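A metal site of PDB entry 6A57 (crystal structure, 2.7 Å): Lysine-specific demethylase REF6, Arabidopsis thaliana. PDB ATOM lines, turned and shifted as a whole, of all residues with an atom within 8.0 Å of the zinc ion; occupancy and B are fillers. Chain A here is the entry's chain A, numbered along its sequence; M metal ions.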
ATOM      1  N   VAL A 107      -4.990  -3.430  16.161  1.00  0.00           N
ATOM      2  CA  VAL A 107      -5.937  -2.369  16.524  1.00  0.00           C
ATOM      3  C   VAL A 107      -5.401  -1.618  17.744  1.00  0.00           C
ATOM      4  O   VAL A 107      -5.134  -2.229  18.779  1.00  0.00           O
ATOM      5  CB  VAL A 107      -7.347  -2.933  16.851  1.00  0.00           C
ATOM      6  CG1 VAL A 107      -8.383  -1.810  16.850  1.00  0.00           C
ATOM      7  CG2 VAL A 107      -7.752  -4.020  15.860  1.00  0.00           C
ATOM      8  N   CYS A 108      -5.227  -0.297  17.597  1.00  0.00           N
ATOM      9  CA  CYS A 108      -4.716   0.521  18.703  1.00  0.00           C
ATOM     10  C   CYS A 108      -5.724   0.544  19.842  1.00  0.00           C
ATOM     11  O   CYS A 108      -6.886   0.901  19.645  1.00  0.00           O
ATOM     12  CB  CYS A 108      -4.425   1.947  18.239  1.00  0.00           C
ATOM     13  SG  CYS A 108      -3.561   2.927  19.481  1.00  0.00           S
ATOM     14  N   ALA A 109      -5.278   0.138  21.024  1.00  0.00           N
ATOM     15  CA  ALA A 109      -6.146   0.033  22.190  1.00  0.00           C
ATOM     16  C   ALA A 109      -6.453   1.399  22.828  1.00  0.00           C
ATOM     17  O   ALA A 109      -7.420   1.514  23.575  1.00  0.00           O
ATOM     18  CB  ALA A 109      -5.526  -0.895  23.232  1.00  0.00           C
ATOM     19  N   GLU A 110      -5.633   2.410  22.539  1.00  0.00           N
ATOM     20  CA  GLU A 110      -5.846   3.757  23.065  1.00  0.00           C
ATOM     21  C   GLU A 110      -7.262   4.200  22.687  1.00  0.00           C
ATOM     22  O   GLU A 110      -7.658   4.015  21.549  1.00  0.00           O
ATOM     23  CB  GLU A 110      -4.811   4.738  22.500  1.00  0.00           C
ATOM     24  CG  GLU A 110      -4.722   6.073  23.241  1.00  0.00           C
ATOM     25  CD  GLU A 110      -4.145   5.946  24.642  1.00  0.00           C
ATOM     26  OE1 GLU A 110      -3.095   5.294  24.820  1.00  0.00           O
ATOM     27  OE2 GLU A 110      -4.752   6.526  25.575  1.00  0.00           O
ATOM     28  N   PRO A 111      -8.040   4.750  23.650  1.00  0.00           N
ATOM     29  CA  PRO A 111      -9.492   4.918  23.404  1.00  0.00           C
ATOM     30  C   PRO A 111      -9.874   5.958  22.331  1.00  0.00           C
ATOM     31  O   PRO A 111     -10.788   5.726  21.549  1.00  0.00           O
ATOM     32  CB  PRO A 111     -10.050   5.328  24.775  1.00  0.00           C
ATOM     33  CG  PRO A 111      -8.950   5.130  25.756  1.00  0.00           C
ATOM     34  CD  PRO A 111      -7.674   5.259  24.986  1.00  0.00           C
ATOM     35  N   ASP A 112      -9.181   7.092  22.319  1.00  0.00           N
ATOM     36  CA  ASP A 112      -9.413   8.121  21.306  1.00  0.00           C
ATOM     37  C   ASP A 112      -9.112   7.587  19.902  1.00  0.00           C
ATOM     38  O   ASP A 112      -9.952   7.649  19.016  1.00  0.00           O
ATOM     39  CB  ASP A 112      -8.546   9.360  21.580  1.00  0.00           C
ATOM     40  N   CYS A 113      -7.892   7.068  19.749  1.00  0.00           N
ATOM     41  CA  CYS A 113      -7.406   6.479  18.493  1.00  0.00           C
ATOM     42  C   CYS A 113      -8.121   5.165  18.191  1.00  0.00           C
ATOM     43  O   CYS A 113      -8.341   4.372  19.098  1.00  0.00           O
ATOM     44  CB  CYS A 113      -5.892   6.235  18.599  1.00  0.00           C
ATOM     45  SG  CYS A 113      -5.119   5.361  17.231  1.00  0.00           S
ATOM     46  N   GLY A 114      -8.478   4.941  16.936  1.00  0.00           N
ATOM     47  CA  GLY A 114      -9.100   3.673  16.524  1.00  0.00           C
ATOM     48  C   GLY A 114      -8.414   3.057  15.317  1.00  0.00           C
ATOM     49  O   GLY A 114      -9.051   2.350  14.531  1.00  0.00           O
ATOM     50  N   GLN A 115      -7.113   3.316  15.185  1.00  0.00           N
ATOM     51  CA  GLN A 115      -6.415   2.990  13.949  1.00  0.00           C
ATOM     52  C   GLN A 115      -6.107   1.501  13.862  1.00  0.00           C
ATOM     53  O   GLN A 115      -5.740   0.883  14.855  1.00  0.00           O
ATOM     54  CB  GLN A 115      -5.117   3.783  13.827  1.00  0.00           C
ATOM     55  CG  GLN A 115      -5.336   5.223  13.413  1.00  0.00           C
ATOM     56  CD  GLN A 115      -4.033   5.952  13.142  1.00  0.00           C
ATOM     57  OE1 GLN A 115      -3.796   7.031  13.672  1.00  0.00           O
ATOM     58  NE2 GLN A 115      -3.181   5.353  12.314  1.00  0.00           N
ATOM     59  N   THR A 116      -6.300   0.961  12.663  1.00  0.00           N
ATOM     60  CA  THR A 116      -5.928  -0.415  12.343  1.00  0.00           C
ATOM     61  C   THR A 116      -4.718  -0.446  11.424  1.00  0.00           C
ATOM     62  O   THR A 116      -4.451   0.502  10.678  1.00  0.00           O
ATOM     63  CB  THR A 116      -7.090  -1.179  11.686  1.00  0.00           C
ATOM     64  OG1 THR A 116      -7.501  -0.524  10.476  1.00  0.00           O
ATOM     65  CG2 THR A 116      -8.264  -1.266  12.641  1.00  0.00           C
ATOM     66  N   PHE A 117      -3.988  -1.558  11.489  1.00  0.00           N
ATOM     67  CA  PHE A 117      -2.768  -1.736  10.712  1.00  0.00           C
ATOM     68  C   PHE A 117      -2.718  -3.152  10.155  1.00  0.00           C
ATOM     69  O   PHE A 117      -3.186  -4.097  10.800  1.00  0.00           O
ATOM     70  CB  PHE A 117      -1.539  -1.503  11.572  1.00  0.00           C
ATOM     71  CG  PHE A 117      -1.500  -0.165  12.236  1.00  0.00           C
ATOM     72  CD1 PHE A 117      -2.223   0.073  13.397  1.00  0.00           C
ATOM     73  CD2 PHE A 117      -0.733   0.867  11.709  1.00  0.00           C
ATOM     74  CE1 PHE A 117      -2.189   1.315  14.020  1.00  0.00           C
ATOM     75  CE2 PHE A 117      -0.691   2.115  12.328  1.00  0.00           C
ATOM     76  CZ  PHE A 117      -1.429   2.334  13.482  1.00  0.00           C
ATOM     77  N   PHE A 123       2.450  -0.877  13.162  1.00  0.00           N
ATOM     78  CA  PHE A 123       1.782  -0.799  14.446  1.00  0.00           C
ATOM     79  C   PHE A 123       2.746  -0.430  15.553  1.00  0.00           C
ATOM     80  O   PHE A 123       2.418   0.407  16.389  1.00  0.00           O
ATOM     81  CB  PHE A 123       1.106  -2.147  14.739  1.00  0.00           C
ATOM     82  CG  PHE A 123       0.285  -2.177  16.000  1.00  0.00           C
ATOM     83  CD1 PHE A 123      -0.594  -1.137  16.315  1.00  0.00           C
ATOM     84  CD2 PHE A 123       0.354  -3.261  16.852  1.00  0.00           C
ATOM     85  CE1 PHE A 123      -1.363  -1.187  17.467  1.00  0.00           C
ATOM     86  CE2 PHE A 123      -0.405  -3.320  18.008  1.00  0.00           C
ATOM     87  CZ  PHE A 123      -1.259  -2.277  18.320  1.00  0.00           C
ATOM     88  N   HIS A 126       3.611   3.292  15.092  1.00  0.00           N
ATOM     89  CA  HIS A 126       2.530   4.154  15.581  1.00  0.00           C
ATOM     90  C   HIS A 126       2.580   4.347  17.097  1.00  0.00           C
ATOM     91  O   HIS A 126       2.426   5.464  17.582  1.00  0.00           O
ATOM     92  CB  HIS A 126       1.156   3.594  15.199  1.00  0.00           C
ATOM     93  CG  HIS A 126       0.025   4.310  15.856  1.00  0.00           C
ATOM     94  ND1 HIS A 126      -0.379   5.577  15.473  1.00  0.00           N
ATOM     95  CD2 HIS A 126      -0.800   3.953  16.869  1.00  0.00           C
ATOM     96  CE1 HIS A 126      -1.397   5.955  16.214  1.00  0.00           C
ATOM     97  NE2 HIS A 126      -1.670   4.995  17.081  1.00  0.00           N
ATOM     98  N   LYS A 127       2.780   3.246  17.826  1.00  0.00           N
ATOM     99  CA  LYS A 127       2.839   3.285  19.278  1.00  0.00           C
ATOM    100  C   LYS A 127       4.095   3.991  19.779  1.00  0.00           C
ATOM    101  O   LYS A 127       4.054   4.718  20.758  1.00  0.00           O
ATOM    102  CB  LYS A 127       2.748   1.882  19.861  1.00  0.00           C
ATOM    103  CG  LYS A 127       1.398   1.228  19.636  1.00  0.00           C
ATOM    104  CD  LYS A 127       1.305  -0.144  20.276  1.00  0.00           C
ATOM    105  CE  LYS A 127       1.954  -1.217  19.437  1.00  0.00           C
ATOM    106  NZ  LYS A 127       1.844  -2.551  20.083  1.00  0.00           N
ATOM    107  N   THR A 130       3.404   7.990  18.897  1.00  0.00           N
ATOM    108  CA  THR A 130       2.323   8.607  19.658  1.00  0.00           C
ATOM    109  C   THR A 130       2.386   8.357  21.177  1.00  0.00           C
ATOM    110  O   THR A 130       1.863   9.141  21.945  1.00  0.00           O
ATOM    111  CB  THR A 130       0.957   8.113  19.176  1.00  0.00           C
ATOM    112  OG1 THR A 130       0.900   6.687  19.311  1.00  0.00           O
ATOM    113  CG2 THR A 130       0.734   8.500  17.728  1.00  0.00           C
ATOM    114  N   GLY A 131       3.019   7.256  21.583  1.00  0.00           N
ATOM    115  CA  GLY A 131       2.921   6.803  22.968  1.00  0.00           C
ATOM    116  C   GLY A 131       1.602   6.127  23.309  1.00  0.00           C
ATOM    117  O   GLY A 131       1.335   5.836  24.475  1.00  0.00           O
ATOM    118  N   HIS A 132       0.782   5.860  22.289  1.00  0.00           N
ATOM    119  CA  HIS A 132      -0.475   5.141  22.461  1.00  0.00           C
ATOM    120  C   HIS A 132      -0.177   3.715  22.889  1.00  0.00           C
ATOM    121  O   HIS A 132       0.807   3.134  22.426  1.00  0.00           O
ATOM    122  CB  HIS A 132      -1.239   5.091  21.141  1.00  0.00           C
ATOM    123  CG  HIS A 132      -1.802   6.411  20.726  1.00  0.00           C
ATOM    124  ND1 HIS A 132      -2.620   6.558  19.615  1.00  0.00           N
ATOM    125  CD2 HIS A 132      -1.696   7.649  21.278  1.00  0.00           C
ATOM    126  CE1 HIS A 132      -2.974   7.824  19.502  1.00  0.00           C
ATOM    127  NE2 HIS A 132      -2.420   8.503  20.490  1.00  0.00           N
ATOM    128  N   SER A 133      -1.004   3.163  23.763  1.00  0.00           N
ATOM    129  CA  SER A 133      -0.921   1.751  24.149  1.00  0.00           C
ATOM    130  C   SER A 133       0.444   1.392  24.770  1.00  0.00           C
ATOM    131  O   SER A 133       0.887   0.249  24.662  1.00  0.00           O
ATOM    132  CB  SER A 133      -1.221   0.872  22.920  1.00  0.00           C
ATOM    133  OG  SER A 133      -1.717  -0.407  23.281  1.00  0.00           O
HETATM  134 ZN    ZN M   1      -3.200   4.948  18.392  1.00  0.00          ZN
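The backbone carbonyl oxygen (O) of His 126 is in hydrogen-bond range of the side-chain hydroxyl (OG1) of Thr 130 (2.6 Å).
The side-chain sulfur of Cys 113 sits close to the backbone NH of Gln 115, 3.5 Å away.
N of Cys 108 sits at hydrogen-bond distance from O of Gln 115, 3.0 Å away.
The backbone NH (N) of His 132 lies close to the side-chain hydroxyl (OG1) of Thr 130.
SG of Cys 108 lies close to N of Glu 110 (3.7 Å).
Within 4 Å of the zinc ion: Cys 108, Cys 113, His 126 and His 132.
Along chain A the residues within 4 Å of the zinc ion span positions 108 to 132.
The nearest printed residue that does not touch the zinc ion is Glu 110 (4.4 Å).
The zinc ion is bound by NE2 of His 126 (2.0 Å), ND1 of His 132 (2.1 Å), SG of Cys 113 (2.3 Å) and SG of Cys 108 (2.3 Å).
The zinc ion has four donor atoms within binding distance.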
